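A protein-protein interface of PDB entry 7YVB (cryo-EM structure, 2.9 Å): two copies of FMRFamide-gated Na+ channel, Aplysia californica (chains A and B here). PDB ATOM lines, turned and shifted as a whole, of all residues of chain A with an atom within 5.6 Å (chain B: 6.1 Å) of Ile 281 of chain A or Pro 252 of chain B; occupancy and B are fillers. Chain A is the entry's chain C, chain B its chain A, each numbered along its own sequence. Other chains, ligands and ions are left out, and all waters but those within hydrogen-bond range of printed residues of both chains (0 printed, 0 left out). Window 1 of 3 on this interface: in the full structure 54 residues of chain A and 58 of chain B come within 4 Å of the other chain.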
ATOM      1  N   ILE A 144      23.857  15.960  23.864  1.00  0.00           N
ATOM      2  CA  ILE A 144      23.112  15.822  25.110  1.00  0.00           C
ATOM      3  C   ILE A 144      23.483  16.929  26.080  1.00  0.00           C
ATOM      4  O   ILE A 144      22.639  17.407  26.845  1.00  0.00           O
ATOM      5  CB  ILE A 144      23.343  14.432  25.722  1.00  0.00           C
ATOM      6  CG1 ILE A 144      22.849  13.351  24.773  1.00  0.00           C
ATOM      7  CG2 ILE A 144      22.615  14.301  27.038  1.00  0.00           C
ATOM      8  CD1 ILE A 144      22.932  11.979  25.354  1.00  0.00           C
ATOM      9  N   ASN A 229      17.080  22.731  26.028  1.00  0.00           N
ATOM     10  CA  ASN A 229      17.741  21.647  26.763  1.00  0.00           C
ATOM     11  C   ASN A 229      18.493  20.719  25.815  1.00  0.00           C
ATOM     12  O   ASN A 229      19.218  19.823  26.255  1.00  0.00           O
ATOM     13  CB  ASN A 229      16.767  20.862  27.673  1.00  0.00           C
ATOM     14  CG  ASN A 229      15.909  19.815  26.949  1.00  0.00           C
ATOM     15  OD1 ASN A 229      16.144  19.443  25.802  1.00  0.00           O
ATOM     16  ND2 ASN A 229      14.886  19.340  27.646  1.00  0.00           N
ATOM     17  N   TYR A 230      18.321  20.928  24.516  1.00  0.00           N
ATOM     18  CA  TYR A 230      19.083  20.252  23.470  1.00  0.00           C
ATOM     19  C   TYR A 230      19.494  21.285  22.434  1.00  0.00           C
ATOM     20  O   TYR A 230      19.249  21.123  21.240  1.00  0.00           O
ATOM     21  CB  TYR A 230      18.291  19.120  22.823  1.00  0.00           C
ATOM     22  CG  TYR A 230      18.331  17.824  23.585  1.00  0.00           C
ATOM     23  CD1 TYR A 230      19.493  17.390  24.192  1.00  0.00           C
ATOM     24  CD2 TYR A 230      17.201  17.033  23.697  1.00  0.00           C
ATOM     25  CE1 TYR A 230      19.529  16.209  24.891  1.00  0.00           C
ATOM     26  CE2 TYR A 230      17.229  15.851  24.393  1.00  0.00           C
ATOM     27  CZ  TYR A 230      18.394  15.443  24.987  1.00  0.00           C
ATOM     28  OH  TYR A 230      18.423  14.261  25.683  1.00  0.00           O
ATOM     29  N   ASN A 279      15.044  16.942  35.777  1.00  0.00           N
ATOM     30  CA  ASN A 279      15.374  16.742  34.371  1.00  0.00           C
ATOM     31  C   ASN A 279      15.941  15.338  34.237  1.00  0.00           C
ATOM     32  O   ASN A 279      17.025  15.055  34.757  1.00  0.00           O
ATOM     33  CB  ASN A 279      16.377  17.790  33.897  1.00  0.00           C
ATOM     34  CG  ASN A 279      16.339  18.001  32.407  1.00  0.00           C
ATOM     35  OD1 ASN A 279      15.457  17.499  31.720  1.00  0.00           O
ATOM     36  ND2 ASN A 279      17.295  18.762  31.896  1.00  0.00           N
ATOM     37  N   ASN A 280      15.216  14.464  33.550  1.00  0.00           N
ATOM     38  CA  ASN A 280      15.567  13.053  33.479  1.00  0.00           C
ATOM     39  C   ASN A 280      16.492  12.711  32.322  1.00  0.00           C
ATOM     40  O   ASN A 280      16.875  11.547  32.184  1.00  0.00           O
ATOM     41  CB  ASN A 280      14.298  12.206  33.371  1.00  0.00           C
ATOM     42  CG  ASN A 280      13.357  12.416  34.527  1.00  0.00           C
ATOM     43  OD1 ASN A 280      13.726  12.994  35.544  1.00  0.00           O
ATOM     44  ND2 ASN A 280      12.130  11.940  34.383  1.00  0.00           N
ATOM     45  N   ILE A 281      16.868  13.680  31.487  1.00  0.00           N
ATOM     46  CA  ILE A 281      17.615  13.368  30.273  1.00  0.00           C
ATOM     47  C   ILE A 281      18.949  14.084  30.172  1.00  0.00           C
ATOM     48  O   ILE A 281      19.828  13.628  29.421  1.00  0.00           O
ATOM     49  CB  ILE A 281      16.762  13.671  29.026  1.00  0.00           C
ATOM     50  CG1 ILE A 281      16.096  15.035  29.165  1.00  0.00           C
ATOM     51  CG2 ILE A 281      15.730  12.600  28.826  1.00  0.00           C
ATOM     52  CD1 ILE A 281      15.217  15.396  28.005  1.00  0.00           C
ATOM     53  N   LEU A 282      19.174  15.185  30.870  1.00  0.00           N
ATOM     54  CA  LEU A 282      20.378  15.969  30.659  1.00  0.00           C
ATOM     55  C   LEU A 282      21.485  15.493  31.593  1.00  0.00           C
ATOM     56  O   LEU A 282      21.380  14.449  32.241  1.00  0.00           O
ATOM     57  CB  LEU A 282      20.075  17.452  30.836  1.00  0.00           C
ATOM     58  CG  LEU A 282      19.819  18.233  29.549  1.00  0.00           C
ATOM     59  CD1 LEU A 282      18.551  17.759  28.873  1.00  0.00           C
ATOM     60  CD2 LEU A 282      19.745  19.717  29.843  1.00  0.00           C
ATOM     61  N   HIS A 283      22.570  16.266  31.659  1.00  0.00           N
ATOM     62  CA  HIS A 283      23.722  15.963  32.506  1.00  0.00           C
ATOM     63  C   HIS A 283      24.354  14.632  32.132  1.00  0.00           C
ATOM     64  O   HIS A 283      24.883  13.920  32.984  1.00  0.00           O
ATOM     65  CB  HIS A 283      23.339  15.990  33.983  1.00  0.00           C
ATOM     66  CG  HIS A 283      22.370  17.074  34.324  1.00  0.00           C
ATOM     67  ND1 HIS A 283      22.727  18.403  34.365  1.00  0.00           N
ATOM     68  CD2 HIS A 283      21.051  17.029  34.620  1.00  0.00           C
ATOM     69  CE1 HIS A 283      21.671  19.129  34.682  1.00  0.00           C
ATOM     70  NE2 HIS A 283      20.641  18.319  34.841  1.00  0.00           N
ATOM     71  N   SER A 284      24.303  14.297  30.851  1.00  0.00           N
ATOM     72  CA  SER A 284      24.846  13.057  30.330  1.00  0.00           C
ATOM     73  C   SER A 284      25.725  13.365  29.129  1.00  0.00           C
ATOM     74  O   SER A 284      25.507  14.350  28.421  1.00  0.00           O
ATOM     75  CB  SER A 284      23.726  12.100  29.939  1.00  0.00           C
ATOM     76  OG  SER A 284      24.227  11.016  29.196  1.00  0.00           O
ATOM     77  N   ARG A 288      22.178  12.655  21.262  1.00  0.00           N
ATOM     78  CA  ARG A 288      20.771  12.288  21.206  1.00  0.00           C
ATOM     79  C   ARG A 288      20.365  12.216  19.741  1.00  0.00           C
ATOM     80  O   ARG A 288      20.385  13.225  19.037  1.00  0.00           O
ATOM     81  CB  ARG A 288      19.924  13.305  21.962  1.00  0.00           C
ATOM     82  CG  ARG A 288      18.473  12.928  22.078  1.00  0.00           C
ATOM     83  CD  ARG A 288      18.249  12.112  23.323  1.00  0.00           C
ATOM     84  NE  ARG A 288      16.841  11.823  23.540  1.00  0.00           N
ATOM     85  CZ  ARG A 288      16.394  11.001  24.481  1.00  0.00           C
ATOM     86  NH1 ARG A 288      17.250  10.392  25.284  1.00  0.00           N
ATOM     87  NH2 ARG A 288      15.095  10.788  24.617  1.00  0.00           N
ATOM     88  N   VAL A 301      13.587  15.150  22.743  1.00  0.00           N
ATOM     89  CA  VAL A 301      13.266  14.698  24.091  1.00  0.00           C
ATOM     90  C   VAL A 301      12.427  13.430  24.034  1.00  0.00           C
ATOM     91  O   VAL A 301      12.832  12.373  24.529  1.00  0.00           O
ATOM     92  CB  VAL A 301      12.551  15.809  24.875  1.00  0.00           C
ATOM     93  CG1 VAL A 301      12.038  15.272  26.192  1.00  0.00           C
ATOM     94  CG2 VAL A 301      13.491  16.974  25.101  1.00  0.00           C
ATOM     95  N   ASP A 302      11.256  13.508  23.404  1.00  0.00           N
ATOM     96  CA  ASP A 302      10.301  12.410  23.479  1.00  0.00           C
ATOM     97  C   ASP A 302      10.724  11.223  22.625  1.00  0.00           C
ATOM     98  O   ASP A 302      10.599  10.071  23.053  1.00  0.00           O
ATOM     99  CB  ASP A 302       8.919  12.899  23.059  1.00  0.00           C
ATOM    100  CG  ASP A 302       8.426  14.047  23.911  1.00  0.00           C
ATOM    101  OD1 ASP A 302       8.005  13.798  25.059  1.00  0.00           O
ATOM    102  OD2 ASP A 302       8.461  15.199  23.436  1.00  0.00           O
ATOM    103  N   THR B 250       4.034  11.224  27.112  1.00  0.00           N
ATOM    104  CA  THR B 250       5.156  10.443  26.622  1.00  0.00           C
ATOM    105  C   THR B 250       6.474  11.084  27.037  1.00  0.00           C
ATOM    106  O   THR B 250       6.517  12.097  27.737  1.00  0.00           O
ATOM    107  CB  THR B 250       5.095  10.309  25.101  1.00  0.00           C
ATOM    108  OG1 THR B 250       5.615  11.498  24.500  1.00  0.00           O
ATOM    109  CG2 THR B 250       3.674  10.119  24.648  1.00  0.00           C
ATOM    110  N   GLY B 251       7.568  10.477  26.593  1.00  0.00           N
ATOM    111  CA  GLY B 251       8.881  11.037  26.779  1.00  0.00           C
ATOM    112  C   GLY B 251       9.486  10.674  28.113  1.00  0.00           C
ATOM    113  O   GLY B 251       8.791  10.291  29.056  1.00  0.00           O
ATOM    114  N   PRO B 252      10.810  10.795  28.217  1.00  0.00           N
ATOM    115  CA  PRO B 252      11.481  10.454  29.476  1.00  0.00           C
ATOM    116  C   PRO B 252      11.208  11.437  30.590  1.00  0.00           C
ATOM    117  O   PRO B 252      11.492  11.120  31.751  1.00  0.00           O
ATOM    118  CB  PRO B 252      12.967  10.447  29.097  1.00  0.00           C
ATOM    119  CG  PRO B 252      13.013  10.579  27.607  1.00  0.00           C
ATOM    120  CD  PRO B 252      11.759  11.245  27.195  1.00  0.00           C
ATOM    121  N   GLU B 253      10.690  12.625  30.283  1.00  0.00           N
ATOM    122  CA  GLU B 253      10.350  13.565  31.342  1.00  0.00           C
ATOM    123  C   GLU B 253       9.152  13.079  32.141  1.00  0.00           C
ATOM    124  O   GLU B 253       9.141  13.169  33.374  1.00  0.00           O
ATOM    125  CB  GLU B 253      10.073  14.941  30.749  1.00  0.00           C
ATOM    126  CG  GLU B 253      11.291  15.596  30.154  1.00  0.00           C
ATOM    127  CD  GLU B 253      12.362  15.859  31.186  1.00  0.00           C
ATOM    128  OE1 GLU B 253      12.023  16.062  32.370  1.00  0.00           O
ATOM    129  OE2 GLU B 253      13.548  15.853  30.812  1.00  0.00           O
ATOM    130  N   ASN B 254       8.136  12.562  31.458  1.00  0.00           N
ATOM    131  CA  ASN B 254       6.935  12.049  32.105  1.00  0.00           C
ATOM    132  C   ASN B 254       7.058  10.532  32.179  1.00  0.00           C
ATOM    133  O   ASN B 254       6.437   9.787  31.425  1.00  0.00           O
ATOM    134  CB  ASN B 254       5.700  12.487  31.338  1.00  0.00           C
ATOM    135  CG  ASN B 254       5.830  13.888  30.799  1.00  0.00           C
ATOM    136  OD1 ASN B 254       6.083  14.829  31.547  1.00  0.00           O
ATOM    137  ND2 ASN B 254       5.685  14.033  29.491  1.00  0.00           N
ATOM    138  N   GLY B 255       7.881  10.077  33.112  1.00  0.00           N
ATOM    139  CA  GLY B 255       8.137   8.658  33.249  1.00  0.00           C
ATOM    140  C   GLY B 255       9.012   8.419  34.453  1.00  0.00           C
ATOM    141  O   GLY B 255       9.436   9.354  35.137  1.00  0.00           O
ATOM    142  N   LEU B 256       9.276   7.146  34.712  1.00  0.00           N
ATOM    143  CA  LEU B 256      10.085   6.788  35.867  1.00  0.00           C
ATOM    144  C   LEU B 256      11.540   7.146  35.611  1.00  0.00           C
ATOM    145  O   LEU B 256      12.076   6.871  34.539  1.00  0.00           O
ATOM    146  CB  LEU B 256       9.945   5.300  36.168  1.00  0.00           C
ATOM    147  CG  LEU B 256      10.541   4.797  37.476  1.00  0.00           C
ATOM    148  CD1 LEU B 256       9.949   5.538  38.651  1.00  0.00           C
ATOM    149  CD2 LEU B 256      10.302   3.312  37.605  1.00  0.00           C
ATOM    150  N   SER B 257      12.176   7.781  36.589  1.00  0.00           N
ATOM    151  CA  SER B 257      13.600   8.069  36.538  1.00  0.00           C
ATOM    152  C   SER B 257      14.205   7.645  37.861  1.00  0.00           C
ATOM    153  O   SER B 257      13.769   8.104  38.920  1.00  0.00           O
ATOM    154  CB  SER B 257      13.866   9.551  36.280  1.00  0.00           C
ATOM    155  OG  SER B 257      15.218   9.872  36.543  1.00  0.00           O
ATOM    156  N   SER B 312      23.387   6.548  31.879  1.00  0.00           N
ATOM    157  CA  SER B 312      21.959   6.823  31.888  1.00  0.00           C
ATOM    158  C   SER B 312      21.337   6.028  30.756  1.00  0.00           C
ATOM    159  O   SER B 312      21.587   6.311  29.583  1.00  0.00           O
ATOM    160  CB  SER B 312      21.685   8.311  31.721  1.00  0.00           C
ATOM    161  OG  SER B 312      20.373   8.524  31.240  1.00  0.00           O
ATOM    162  N   SER B 314      17.936   4.806  28.902  1.00  0.00           N
ATOM    163  CA  SER B 314      16.548   5.169  28.685  1.00  0.00           C
ATOM    164  C   SER B 314      15.864   4.010  27.981  1.00  0.00           C
ATOM    165  O   SER B 314      16.307   3.577  26.913  1.00  0.00           O
ATOM    166  CB  SER B 314      16.444   6.447  27.859  1.00  0.00           C
ATOM    167  OG  SER B 314      17.142   7.507  28.485  1.00  0.00           O
ATOM    168  N   ARG B 529      21.768   6.101  36.003  1.00  0.00           N
ATOM    169  CA  ARG B 529      20.417   6.611  35.851  1.00  0.00           C
ATOM    170  C   ARG B 529      19.652   5.690  34.921  1.00  0.00           C
ATOM    171  O   ARG B 529      20.204   5.176  33.949  1.00  0.00           O
ATOM    172  CB  ARG B 529      20.406   8.036  35.303  1.00  0.00           C
ATOM    173  CG  ARG B 529      19.019   8.635  35.242  1.00  0.00           C
ATOM    174  CD  ARG B 529      19.057  10.096  34.888  1.00  0.00           C
ATOM    175  NE  ARG B 529      19.595  10.316  33.555  1.00  0.00           N
ATOM    176  CZ  ARG B 529      20.148  11.453  33.158  1.00  0.00           C
ATOM    177  NH1 ARG B 529      20.614  11.570  31.927  1.00  0.00           N
ATOM    178  NH2 ARG B 529      20.233  12.473  33.997  1.00  0.00           N
ATOM    179  N   ASN B 531      15.916   5.711  33.016  1.00  0.00           N
ATOM    180  CA  ASN B 531      14.621   6.273  32.669  1.00  0.00           C
ATOM    181  C   ASN B 531      13.806   5.183  32.003  1.00  0.00           C
ATOM    182  O   ASN B 531      14.331   4.436  31.183  1.00  0.00           O
ATOM    183  CB  ASN B 531      14.762   7.476  31.740  1.00  0.00           C
ATOM    184  CG  ASN B 531      15.703   8.517  32.281  1.00  0.00           C
ATOM    185  OD1 ASN B 531      15.601   8.918  33.436  1.00  0.00           O
ATOM    186  ND2 ASN B 531      16.629   8.964  31.449  1.00  0.00           N
ATOM    187  N   ILE B 532      12.547   5.058  32.396  1.00  0.00           N
ATOM    188  CA  ILE B 532      11.615   4.131  31.770  1.00  0.00           C
ATOM    189  C   ILE B 532      10.364   4.916  31.432  1.00  0.00           C
ATOM    190  O   ILE B 532       9.736   5.502  32.321  1.00  0.00           O
ATOM    191  CB  ILE B 532      11.285   2.936  32.674  1.00  0.00           C
ATOM    192  CG1 ILE B 532      12.557   2.165  32.992  1.00  0.00           C
ATOM    193  CG2 ILE B 532      10.292   2.031  31.998  1.00  0.00           C
ATOM    194  CD1 ILE B 532      12.361   1.063  33.957  1.00  0.00           C
ATOM    195  N   TYR B 533      10.004   4.935  30.153  1.00  0.00           N
ATOM    196  CA  TYR B 533       8.958   5.836  29.711  1.00  0.00           C
ATOM    197  C   TYR B 533       8.258   5.246  28.503  1.00  0.00           C
ATOM    198  O   TYR B 533       8.748   4.310  27.869  1.00  0.00           O
ATOM    199  CB  TYR B 533       9.521   7.213  29.370  1.00  0.00           C
ATOM    200  CG  TYR B 533      10.608   7.182  28.322  1.00  0.00           C
ATOM    201  CD1 TYR B 533      11.935   7.037  28.678  1.00  0.00           C
ATOM    202  CD2 TYR B 533      10.305   7.313  26.977  1.00  0.00           C
ATOM    203  CE1 TYR B 533      12.923   7.010  27.730  1.00  0.00           C
ATOM    204  CE2 TYR B 533      11.288   7.289  26.023  1.00  0.00           C
ATOM    205  CZ  TYR B 533      12.596   7.137  26.404  1.00  0.00           C
ATOM    206  OH  TYR B 533      13.583   7.114  25.451  1.00  0.00           O
ATOM    207  N   LEU B 534       7.102   5.814  28.192  1.00  0.00           N
ATOM    208  CA  LEU B 534       6.359   5.456  26.997  1.00  0.00           C
ATOM    209  C   LEU B 534       6.809   6.367  25.863  1.00  0.00           C
ATOM    210  O   LEU B 534       6.716   7.591  25.978  1.00  0.00           O
ATOM    211  CB  LEU B 534       4.856   5.592  27.233  1.00  0.00           C
ATOM    212  CG  LEU B 534       4.081   4.463  27.921  1.00  0.00           C
ATOM    213  CD1 LEU B 534       4.142   3.188  27.112  1.00  0.00           C
ATOM    214  CD2 LEU B 534       4.569   4.226  29.334  1.00  0.00           C
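The side-chain amide nitrogen (ND2) of Asn 531 of chain B sits at hydrogen-bond distance from the backbone carbonyl oxygen (O) of Asn 280 of chain A (2.7 Å). NH2 of Arg 529 of chain B lies within hydrogen-bond range of O of Leu 282 of chain A, 2.9 Å away. The backbone carbonyl oxygen of Pro 252 of chain B lies within hydrogen-bond range of the side-chain amide nitrogen of Asn 280 of chain A (2.8 Å). The backbone carbonyl oxygen (O) of Asn 280 of chain A lies within hydrogen-bond range of the guanidinium group (NE) of Arg 529 of chain B. The backbone carbonyl oxygen of Glu 253 of chain B is in hydrogen-bond range of the side-chain amide nitrogen of Asn 280 of chain A (3.4 Å). The guanidinium group (NH1) of Arg 529 of chain B is in hydrogen-bond range of the backbone carbonyl oxygen (O) of Ile 281 of chain A (3.3 Å). OD1 of Asp 302 of chain A is in hydrogen-bond range of OG1 of Thr 250 of chain B (3.4 Å). The side-chain carboxylate of Glu 253 of chain B lies close to the side-chain amide oxygen of Asn 279 of chain A, 2.7 Å away.
OG of Ser 314 of chain B sits at hydrogen-bond distance from ND2 of Asn 531 of chain B (3.3 Å). The backbone NH (N) of Gly 251 of chain B lies within hydrogen-bond range of the backbone carbonyl oxygen (O) of Leu 534 of chain B, 3.1 Å away. The guanidinium group of Arg 288 of chain A sits at hydrogen-bond distance from the backbone carbonyl oxygen of Val 301 of chain A. O of Thr 250 of chain B is in hydrogen-bond range of ND2 of Asn 254 of chain B, 2.7 Å away. The side-chain hydroxyl (OG) of Ser 312 of chain B lies within hydrogen-bond range of the guanidinium group (NE) of Arg 529 of chain B. OG of Ser 257 of chain B is in hydrogen-bond range of OD1 of Asn 531 of chain B (3.3 Å).
Among the printed residues, merely in contact across the chains: Val 301 of chain A with Pro 252 of chain B, Ile 281 of chain A with Glu 253 of chain B, Asp 302 of chain A with Gly 251 of chain B, Asn 280 of chain A with Ser 257 of chain B, Ile 281 of chain A with Pro 252 of chain B, Arg 288 of chain A with Pro 252 of chain B, Ser 284 of chain A with Arg 529 of chain B and Asn 280 of chain A with Gly 255 of chain B.
Ile 144 of chain A touches none of the printed residues of chain B. Of the printed residues of chain B, Asn 279 of chain A touches Glu 253 (2.7 Å). Of chain B, only Pro 252, Glu 253 and Arg 529 come within 4 Å of Ile 281 of chain A. Printed residues of chain B within 4 Å of Leu 282 of chain A: Arg 529 (2.9 Å). Of the printed residues of chain B, Val 301 of chain A touches Pro 252 (3.1 Å). Of the printed residues of chain A, Gly 251 of chain B touches Asp 302. Pro 252 of chain B touches four residues of chain A. Of the printed residues of chain A, Glu 253 of chain B touches Asn 279 (2.7 Å), Asn 280 (3.4 Å) and Ile 281 (3.1 Å). Leu 256 of chain B touches none of the printed residues of chain A. The nearest printed residue of chain B that does not touch Asp 302 of chain A is Tyr 533 of chain B (4.1 Å).
Of the 15 printed residues of chain B, 8 touch a printed residue of chain A. Printed residues of chain B that touch a printed residue of chain A: Thr 250, Gly 251, Pro 252, Glu 253, Gly 255, Ser 257, Arg 529 and Asn 531. Hydrophobic or aromatic side chains of chain B within 4 Å of the printed part of chain A: Pro 252. Among the printed residues, 16 pairs touch across the chains. Among the printed residues, no Asp or Glu carboxylate lies within 4 Å of a Lys or Arg side-chain nitrogen of the other chain.
No position is printed for both chains. Of the 16 pairs that touch across the chains among the printed residues, none has its exchanged pair printed and touching as well.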
